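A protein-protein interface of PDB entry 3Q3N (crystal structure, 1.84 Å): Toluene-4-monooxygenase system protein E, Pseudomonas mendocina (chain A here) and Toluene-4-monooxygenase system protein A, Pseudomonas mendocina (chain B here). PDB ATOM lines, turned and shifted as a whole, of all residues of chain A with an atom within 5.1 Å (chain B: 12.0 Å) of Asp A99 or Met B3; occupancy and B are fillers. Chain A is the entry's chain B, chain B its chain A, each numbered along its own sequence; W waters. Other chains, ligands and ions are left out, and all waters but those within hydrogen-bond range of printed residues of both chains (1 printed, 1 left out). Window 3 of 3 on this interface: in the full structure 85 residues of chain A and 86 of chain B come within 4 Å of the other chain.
Water W1 lies within hydrogen-bond range of O of Gln A95 (3.1 Å) and SD of Met B3 (3.5 Å).
OD1 of Asp A99 is in hydrogen-bond range of N of Ala B2, 2.7 Å away. ND2 of Asn A102 lies close to N of Ala B2. The side-chain carboxylate (OE1) of Glu A103 lies within hydrogen-bond range of the backbone NH (N) of Ala B2, 2.6 Å away. The side-chain sulfur (SD) of Met B3 sits close to the backbone NH (N) of Asp A99, 3.7 Å away. SD of Met B3 lies close to OH of Tyr A168 (3.7 Å). N of His B4 is in hydrogen-bond range of OH of Tyr A168 (3.0 Å). SD of Met B3 lies close to O of Gln A95 (3.6 Å).
Among the printed residues, merely in contact across the chains: Tyr A168 with Trp B9 (3.4 Å), Gln A95 with Pro B56 (3.5 Å) and Asn A102 with His B4 (3.5 Å).
Printed residues of chain B within 4 Å of Asp A99: Ala B2 and Met B3. Met B3 touches just these residues of chain A: Gln A95 (3.1 Å), Asp A99 (3.6 Å) and Tyr A168 (3.4 Å). Of chain B, only Met B3 and Pro B56 come within 4 Å of Gln A95. No residue of chain B comes within 4 Å of Ser A96. No residue of chain B comes within 4 Å of Phe A98. Of the printed residues of chain B, Asn A102 touches Ala B2 and His B4. Of chain B, only Ala B2 comes within 4 Å of Glu A103. Of the printed residues of chain A, Trp B9 touches Tyr A168. Printed residues of chain A within 4 Å of Pro B56: Gln A95. Printed residues of chain A within 4 Å of His B4: Asn A102 (3.5 Å) and Tyr A168 (3.0 Å). The nearest residue of chain B that does not touch Asp A99 is His B4 (7.3 Å).
The backbone carbonyl oxygen of His B4 lies within hydrogen-bond range of the indole nitrogen of Trp B9. The indole nitrogen of Trp B9 lies close to the backbone carbonyl oxygen of Pro B5, 3.2 Å away.
Of the 14 printed residues of chain B, 5 touch a printed residue of chain A. Printed residues of chain B that touch a printed residue of chain A: Ala B2, Met B3, His B4, Trp B9 and Pro B56. Hydrophobic or aromatic side chains of chain B that line the printed part of chain A: Ala B2, Met B3, His B4, Trp B9 and Pro B56. Printed residues of chain A that touch a printed residue of chain B: Gln A95, Asp A99, Asn A102, Glu A103 and Tyr A168. Among the printed residues, 10 pairs touch across the chains.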
ATOM      1  N   GLN A  95     -26.826 -21.751  32.688  1.00  0.00           N
ATOM      2  CA  GLN A  95     -25.973 -22.183  31.578  1.00  0.00           C
ATOM      3  C   GLN A  95     -25.542 -23.642  31.784  1.00  0.00           C
ATOM      4  O   GLN A  95     -25.398 -24.399  30.823  1.00  0.00           O
ATOM      5  CB  GLN A  95     -24.765 -21.262  31.435  1.00  0.00           C
ATOM      6  CG  GLN A  95     -25.151 -19.786  31.204  1.00  0.00           C
ATOM      7  CD  GLN A  95     -25.745 -19.521  29.819  1.00  0.00           C
ATOM      8  OE1 GLN A  95     -26.782 -18.855  29.682  1.00  0.00           O
ATOM      9  NE2 GLN A  95     -25.079 -20.020  28.792  1.00  0.00           N
ATOM     10  N   SER A  96     -25.364 -24.040  33.043  1.00  0.00           N
ATOM     11  CA  SER A  96     -25.016 -25.424  33.359  1.00  0.00           C
ATOM     12  C   SER A  96     -26.155 -26.381  33.035  1.00  0.00           C
ATOM     13  O   SER A  96     -25.922 -27.484  32.524  1.00  0.00           O
ATOM     14  CB  SER A  96     -24.594 -25.568  34.827  1.00  0.00           C
ATOM     15  OG  SER A  96     -23.281 -25.063  35.007  1.00  0.00           O
ATOM     16  N   LEU A  97     -27.381 -25.961  33.331  1.00  0.00           N
ATOM     17  CA  LEU A  97     -28.562 -26.709  32.914  1.00  0.00           C
ATOM     18  C   LEU A  97     -28.588 -26.862  31.393  1.00  0.00           C
ATOM     19  O   LEU A  97     -28.820 -27.959  30.880  1.00  0.00           O
ATOM     20  CB  LEU A  97     -29.846 -26.011  33.369  1.00  0.00           C
ATOM     21  CG  LEU A  97     -30.158 -26.005  34.868  1.00  0.00           C
ATOM     22  CD1 LEU A  97     -31.344 -25.107  35.155  1.00  0.00           C
ATOM     23  CD2 LEU A  97     -30.429 -27.426  35.356  1.00  0.00           C
ATOM     24  N   PHE A  98     -28.385 -25.758  30.671  1.00  0.00           N
ATOM     25  CA  PHE A  98     -28.386 -25.814  29.198  1.00  0.00           C
ATOM     26  C   PHE A  98     -27.392 -26.874  28.690  1.00  0.00           C
ATOM     27  O   PHE A  98     -27.720 -27.703  27.827  1.00  0.00           O
ATOM     28  CB  PHE A  98     -28.029 -24.452  28.582  1.00  0.00           C
ATOM     29  CG  PHE A  98     -29.115 -23.401  28.698  1.00  0.00           C
ATOM     30  CD1 PHE A  98     -28.857 -22.088  28.317  1.00  0.00           C
ATOM     31  CD2 PHE A  98     -30.379 -23.714  29.170  1.00  0.00           C
ATOM     32  CE1 PHE A  98     -29.844 -21.104  28.409  1.00  0.00           C
ATOM     33  CE2 PHE A  98     -31.365 -22.738  29.273  1.00  0.00           C
ATOM     34  CZ  PHE A  98     -31.103 -21.434  28.885  1.00  0.00           C
ATOM     35  N   ASP A  99     -26.174 -26.829  29.227  1.00  0.00           N
ATOM     36  CA  ASP A  99     -25.102 -27.730  28.819  1.00  0.00           C
ATOM     37  C   ASP A  99     -25.492 -29.178  29.068  1.00  0.00           C
ATOM     38  O   ASP A  99     -25.378 -30.024  28.185  1.00  0.00           O
ATOM     39  CB  ASP A  99     -23.827 -27.383  29.581  1.00  0.00           C
ATOM     40  CG  ASP A  99     -22.613 -28.145  29.084  1.00  0.00           C
ATOM     41  OD1 ASP A  99     -22.617 -28.614  27.928  1.00  0.00           O
ATOM     42  OD2 ASP A  99     -21.638 -28.254  29.854  1.00  0.00           O
ATOM     43  N   GLN A 100     -25.979 -29.447  30.276  1.00  0.00           N
ATOM     44  CA  GLN A 100     -26.283 -30.798  30.719  1.00  0.00           C
ATOM     45  C   GLN A 100     -27.495 -31.395  30.010  1.00  0.00           C
ATOM     46  O   GLN A 100     -27.504 -32.584  29.663  1.00  0.00           O
ATOM     47  CB  GLN A 100     -26.488 -30.788  32.237  1.00  0.00           C
ATOM     48  CG  GLN A 100     -27.388 -31.875  32.749  1.00  0.00           C
ATOM     49  CD  GLN A 100     -26.655 -33.181  32.944  1.00  0.00           C
ATOM     50  OE1 GLN A 100     -25.497 -33.332  32.543  1.00  0.00           O
ATOM     51  NE2 GLN A 100     -27.326 -34.133  33.576  1.00  0.00           N
ATOM     52  N   PHE A 101     -28.519 -30.577  29.786  1.00  0.00           N
ATOM     53  CA  PHE A 101     -29.707 -31.069  29.105  1.00  0.00           C
ATOM     54  C   PHE A 101     -29.424 -31.303  27.632  1.00  0.00           C
ATOM     55  O   PHE A 101     -29.948 -32.238  27.027  1.00  0.00           O
ATOM     56  CB  PHE A 101     -30.900 -30.136  29.334  1.00  0.00           C
ATOM     57  CG  PHE A 101     -31.568 -30.345  30.672  1.00  0.00           C
ATOM     58  CD1 PHE A 101     -32.867 -30.834  30.748  1.00  0.00           C
ATOM     59  CD2 PHE A 101     -30.880 -30.099  31.849  1.00  0.00           C
ATOM     60  CE1 PHE A 101     -33.482 -31.042  31.973  1.00  0.00           C
ATOM     61  CE2 PHE A 101     -31.485 -30.305  33.081  1.00  0.00           C
ATOM     62  CZ  PHE A 101     -32.789 -30.779  33.142  1.00  0.00           C
ATOM     63  N   ASN A 102     -28.570 -30.465  27.055  1.00  0.00           N
ATOM     64  CA  ASN A 102     -28.165 -30.659  25.670  1.00  0.00           C
ATOM     65  C   ASN A 102     -27.333 -31.943  25.519  1.00  0.00           C
ATOM     66  O   ASN A 102     -27.473 -32.683  24.537  1.00  0.00           O
ATOM     67  CB  ASN A 102     -27.410 -29.426  25.155  1.00  0.00           C
ATOM     68  CG  ASN A 102     -26.682 -29.691  23.852  1.00  0.00           C
ATOM     69  OD1 ASN A 102     -27.175 -29.361  22.762  1.00  0.00           O
ATOM     70  ND2 ASN A 102     -25.505 -30.296  23.953  1.00  0.00           N
ATOM     71  N   GLU A 103     -26.473 -32.210  26.502  1.00  0.00           N
ATOM     72  CA  GLU A 103     -25.690 -33.444  26.515  1.00  0.00           C
ATOM     73  C   GLU A 103     -26.611 -34.653  26.545  1.00  0.00           C
ATOM     74  O   GLU A 103     -26.352 -35.663  25.890  1.00  0.00           O
ATOM     75  CB  GLU A 103     -24.762 -33.491  27.734  1.00  0.00           C
ATOM     76  CG  GLU A 103     -23.494 -32.672  27.595  1.00  0.00           C
ATOM     77  CD  GLU A 103     -22.658 -33.113  26.406  1.00  0.00           C
ATOM     78  OE1 GLU A 103     -22.399 -32.276  25.519  1.00  0.00           O
ATOM     79  OE2 GLU A 103     -22.272 -34.301  26.361  1.00  0.00           O
ATOM     80  N   TYR A 168     -31.236 -17.886  22.998  1.00  0.00           N
ATOM     81  CA  TYR A 168     -30.359 -19.054  23.001  1.00  0.00           C
ATOM     82  C   TYR A 168     -31.162 -20.345  22.787  1.00  0.00           C
ATOM     83  O   TYR A 168     -30.776 -21.207  21.999  1.00  0.00           O
ATOM     84  CB  TYR A 168     -29.576 -19.127  24.316  1.00  0.00           C
ATOM     85  CG  TYR A 168     -28.591 -20.269  24.384  1.00  0.00           C
ATOM     86  CD1 TYR A 168     -27.263 -20.084  24.021  1.00  0.00           C
ATOM     87  CD2 TYR A 168     -28.990 -21.535  24.806  1.00  0.00           C
ATOM     88  CE1 TYR A 168     -26.358 -21.119  24.074  1.00  0.00           C
ATOM     89  CE2 TYR A 168     -28.085 -22.583  24.858  1.00  0.00           C
ATOM     90  CZ  TYR A 168     -26.774 -22.363  24.495  1.00  0.00           C
ATOM     91  OH  TYR A 168     -25.869 -23.392  24.546  1.00  0.00           O
ATOM     92  N   ALA B   2     -23.306 -29.794  25.615  1.00  0.00           N
ATOM     93  CA  ALA B   2     -22.491 -28.817  24.913  1.00  0.00           C
ATOM     94  C   ALA B   2     -23.190 -27.467  24.898  1.00  0.00           C
ATOM     95  O   ALA B   2     -24.400 -27.384  25.124  1.00  0.00           O
ATOM     96  CB  ALA B   2     -22.192 -29.284  23.480  1.00  0.00           C
ATOM     97  N   MET B   3     -22.418 -26.418  24.623  1.00  0.00           N
ATOM     98  CA  MET B   3     -22.940 -25.055  24.528  1.00  0.00           C
ATOM     99  C   MET B   3     -22.735 -24.569  23.102  1.00  0.00           C
ATOM    100  O   MET B   3     -21.769 -24.961  22.443  1.00  0.00           O
ATOM    101  CB  MET B   3     -22.187 -24.111  25.468  1.00  0.00           C
ATOM    102  CG  MET B   3     -22.246 -24.493  26.940  1.00  0.00           C
ATOM    103  SD  MET B   3     -23.937 -24.471  27.525  1.00  0.00           S
ATOM    104  CE  MET B   3     -24.299 -22.710  27.485  1.00  0.00           C
ATOM    105  N   HIS B   4     -23.625 -23.709  22.624  1.00  0.00           N
ATOM    106  CA  HIS B   4     -23.482 -23.183  21.266  1.00  0.00           C
ATOM    107  C   HIS B   4     -22.845 -21.807  21.312  1.00  0.00           C
ATOM    108  O   HIS B   4     -23.134 -21.022  22.211  1.00  0.00           O
ATOM    109  CB  HIS B   4     -24.838 -23.209  20.565  1.00  0.00           C
ATOM    110  CG  HIS B   4     -25.525 -24.524  20.729  1.00  0.00           C
ATOM    111  ND1 HIS B   4     -26.593 -24.708  21.579  1.00  0.00           N
ATOM    112  CD2 HIS B   4     -25.209 -25.751  20.251  1.00  0.00           C
ATOM    113  CE1 HIS B   4     -26.942 -25.983  21.573  1.00  0.00           C
ATOM    114  NE2 HIS B   4     -26.116 -26.638  20.778  1.00  0.00           N
ATOM    115  N   PRO B   5     -21.937 -21.533  20.366  1.00  0.00           N
ATOM    116  CA  PRO B   5     -21.153 -20.296  20.361  1.00  0.00           C
ATOM    117  C   PRO B   5     -22.021 -19.062  20.110  1.00  0.00           C
ATOM    118  O   PRO B   5     -22.995 -19.120  19.362  1.00  0.00           O
ATOM    119  CB  PRO B   5     -20.169 -20.501  19.200  1.00  0.00           C
ATOM    120  CG  PRO B   5     -20.808 -21.516  18.326  1.00  0.00           C
ATOM    121  CD  PRO B   5     -21.592 -22.418  19.240  1.00  0.00           C
ATOM    122  N   ARG B   6     -21.651 -17.953  20.734  1.00  0.00           N
ATOM    123  CA  ARG B   6     -22.423 -16.717  20.622  1.00  0.00           C
ATOM    124  C   ARG B   6     -22.764 -16.345  19.173  1.00  0.00           C
ATOM    125  O   ARG B   6     -23.870 -15.881  18.893  1.00  0.00           O
ATOM    126  CB  ARG B   6     -21.687 -15.561  21.308  1.00  0.00           C
ATOM    127  CG  ARG B   6     -22.512 -14.271  21.408  1.00  0.00           C
ATOM    128  CD  ARG B   6     -21.712 -13.171  22.122  1.00  0.00           C
ATOM    129  NE  ARG B   6     -20.645 -12.646  21.268  1.00  0.00           N
ATOM    130  CZ  ARG B   6     -19.592 -11.954  21.705  1.00  0.00           C
ATOM    131  NH1 ARG B   6     -19.441 -11.700  22.995  1.00  0.00           N
ATOM    132  NH2 ARG B   6     -18.682 -11.519  20.842  1.00  0.00           N
ATOM    133  N   LYS B   7     -21.833 -16.550  18.246  1.00  0.00           N
ATOM    134  CA  LYS B   7     -22.089 -16.138  16.863  1.00  0.00           C
ATOM    135  C   LYS B   7     -23.331 -16.804  16.268  1.00  0.00           C
ATOM    136  O   LYS B   7     -23.968 -16.245  15.377  1.00  0.00           O
ATOM    137  CB  LYS B   7     -20.875 -16.383  15.962  1.00  0.00           C
ATOM    138  CG  LYS B   7     -20.547 -17.860  15.749  1.00  0.00           C
ATOM    139  CD  LYS B   7     -19.286 -18.039  14.910  1.00  0.00           C
ATOM    140  CE  LYS B   7     -18.802 -19.485  14.939  1.00  0.00           C
ATOM    141  NZ  LYS B   7     -19.827 -20.450  14.435  1.00  0.00           N
ATOM    142  N   ASP B   8     -23.674 -17.991  16.762  1.00  0.00           N
ATOM    143  CA  ASP B   8     -24.798 -18.754  16.224  1.00  0.00           C
ATOM    144  C   ASP B   8     -26.162 -18.271  16.722  1.00  0.00           C
ATOM    145  O   ASP B   8     -27.185 -18.546  16.095  1.00  0.00           O
ATOM    146  CB  ASP B   8     -24.655 -20.241  16.559  1.00  0.00           C
ATOM    147  CG  ASP B   8     -23.480 -20.895  15.862  1.00  0.00           C
ATOM    148  OD1 ASP B   8     -22.908 -20.283  14.939  1.00  0.00           O
ATOM    149  OD2 ASP B   8     -23.143 -22.037  16.232  1.00  0.00           O
ATOM    150  N   TRP B   9     -26.193 -17.581  17.854  1.00  0.00           N
ATOM    151  CA  TRP B   9     -27.473 -17.123  18.401  1.00  0.00           C
ATOM    152  C   TRP B   9     -27.521 -15.611  18.637  1.00  0.00           C
ATOM    153  O   TRP B   9     -28.561 -15.084  19.022  1.00  0.00           O
ATOM    154  CB  TRP B   9     -27.838 -17.871  19.703  1.00  0.00           C
ATOM    155  CG  TRP B   9     -26.711 -17.961  20.725  1.00  0.00           C
ATOM    156  CD1 TRP B   9     -25.822 -18.990  20.869  1.00  0.00           C
ATOM    157  CD2 TRP B   9     -26.361 -16.990  21.728  1.00  0.00           C
ATOM    158  NE1 TRP B   9     -24.942 -18.720  21.887  1.00  0.00           N
ATOM    159  CE2 TRP B   9     -25.245 -17.497  22.428  1.00  0.00           C
ATOM    160  CE3 TRP B   9     -26.868 -15.735  22.085  1.00  0.00           C
ATOM    161  CZ2 TRP B   9     -24.635 -16.800  23.482  1.00  0.00           C
ATOM    162  CZ3 TRP B   9     -26.258 -15.038  23.135  1.00  0.00           C
ATOM    163  CH2 TRP B   9     -25.154 -15.579  23.816  1.00  0.00           C
ATOM    164  N   TYR B  10     -26.414 -14.912  18.394  1.00  0.00           N
ATOM    165  CA  TYR B  10     -26.379 -13.474  18.696  1.00  0.00           C
ATOM    166  C   TYR B  10     -27.444 -12.686  17.941  1.00  0.00           C
ATOM    167  O   TYR B  10     -28.039 -11.757  18.494  1.00  0.00           O
ATOM    168  CB  TYR B  10     -24.987 -12.861  18.435  1.00  0.00           C
ATOM    169  CG  TYR B  10     -24.888 -11.441  18.962  1.00  0.00           C
ATOM    170  CD1 TYR B  10     -24.573 -11.195  20.290  1.00  0.00           C
ATOM    171  CD2 TYR B  10     -25.162 -10.352  18.147  1.00  0.00           C
ATOM    172  CE1 TYR B  10     -24.498  -9.900  20.784  1.00  0.00           C
ATOM    173  CE2 TYR B  10     -25.085  -9.052  18.639  1.00  0.00           C
ATOM    174  CZ  TYR B  10     -24.757  -8.841  19.955  1.00  0.00           C
ATOM    175  OH  TYR B  10     -24.700  -7.558  20.456  1.00  0.00           O
ATOM    176  N   SER B  54     -22.754 -10.456  25.870  1.00  0.00           N
ATOM    177  CA  SER B  54     -24.050 -11.081  26.108  1.00  0.00           C
ATOM    178  C   SER B  54     -24.224 -11.182  27.614  1.00  0.00           C
ATOM    179  O   SER B  54     -23.240 -11.130  28.351  1.00  0.00           O
ATOM    180  CB  SER B  54     -24.085 -12.475  25.481  1.00  0.00           C
ATOM    181  OG  SER B  54     -23.167 -13.347  26.131  1.00  0.00           O
ATOM    182  N   TYR B  55     -25.459 -11.331  28.073  1.00  0.00           N
ATOM    183  CA  TYR B  55     -25.735 -11.304  29.513  1.00  0.00           C
ATOM    184  C   TYR B  55     -24.855 -12.250  30.376  1.00  0.00           C
ATOM    185  O   TYR B  55     -24.236 -11.811  31.353  1.00  0.00           O
ATOM    186  CB  TYR B  55     -27.239 -11.505  29.786  1.00  0.00           C
ATOM    187  CG  TYR B  55     -27.575 -11.319  31.247  1.00  0.00           C
ATOM    188  CD1 TYR B  55     -27.483 -12.381  32.143  1.00  0.00           C
ATOM    189  CD2 TYR B  55     -27.941 -10.077  31.738  1.00  0.00           C
ATOM    190  CE1 TYR B  55     -27.776 -12.211  33.491  1.00  0.00           C
ATOM    191  CE2 TYR B  55     -28.238  -9.889  33.105  1.00  0.00           C
ATOM    192  CZ  TYR B  55     -28.147 -10.965  33.966  1.00  0.00           C
ATOM    193  OH  TYR B  55     -28.429 -10.805  35.306  1.00  0.00           O
ATOM    194  N   PRO B  56     -24.790 -13.550  30.030  1.00  0.00           N
ATOM    195  CA  PRO B  56     -23.982 -14.436  30.876  1.00  0.00           C
ATOM    196  C   PRO B  56     -22.512 -14.013  30.958  1.00  0.00           C
ATOM    197  O   PRO B  56     -21.916 -14.117  32.030  1.00  0.00           O
ATOM    198  CB  PRO B  56     -24.088 -15.806  30.167  1.00  0.00           C
ATOM    199  CG  PRO B  56     -25.301 -15.707  29.305  1.00  0.00           C
ATOM    200  CD  PRO B  56     -25.397 -14.264  28.892  1.00  0.00           C
ATOM    201  N   GLU B  57     -21.927 -13.570  29.843  1.00  0.00           N
ATOM    202  CA  GLU B  57     -20.518 -13.157  29.853  1.00  0.00           C
ATOM    203  C   GLU B  57     -20.361 -11.877  30.659  1.00  0.00           C
ATOM    204  O   GLU B  57     -19.373 -11.681  31.368  1.00  0.00           O
ATOM    205  CB  GLU B  57     -20.056 -12.890  28.416  1.00  0.00           C
ATOM    206  CG  GLU B  57     -20.182 -14.087  27.516  1.00  0.00           C
ATOM    207  CD  GLU B  57     -19.872 -13.731  26.069  1.00  0.00           C
ATOM    208  OE1 GLU B  57     -20.665 -12.997  25.438  1.00  0.00           O
ATOM    209  OE2 GLU B  57     -18.819 -14.177  25.578  1.00  0.00           O
ATOM    210  N   SER B  60     -20.434 -12.373  34.498  1.00  0.00           N
ATOM    211  CA  SER B  60     -19.245 -13.116  34.887  1.00  0.00           C
ATOM    212  C   SER B  60     -17.962 -12.277  34.821  1.00  0.00           C
ATOM    213  O   SER B  60     -17.148 -12.279  35.748  1.00  0.00           O
ATOM    214  CB  SER B  60     -19.085 -14.351  33.995  1.00  0.00           C
ATOM    215  OG  SER B  60     -17.880 -15.030  34.320  1.00  0.00           O
HETATM  216  O   HOH W   1     -22.396 -23.725  30.600  1.00  0.00           O
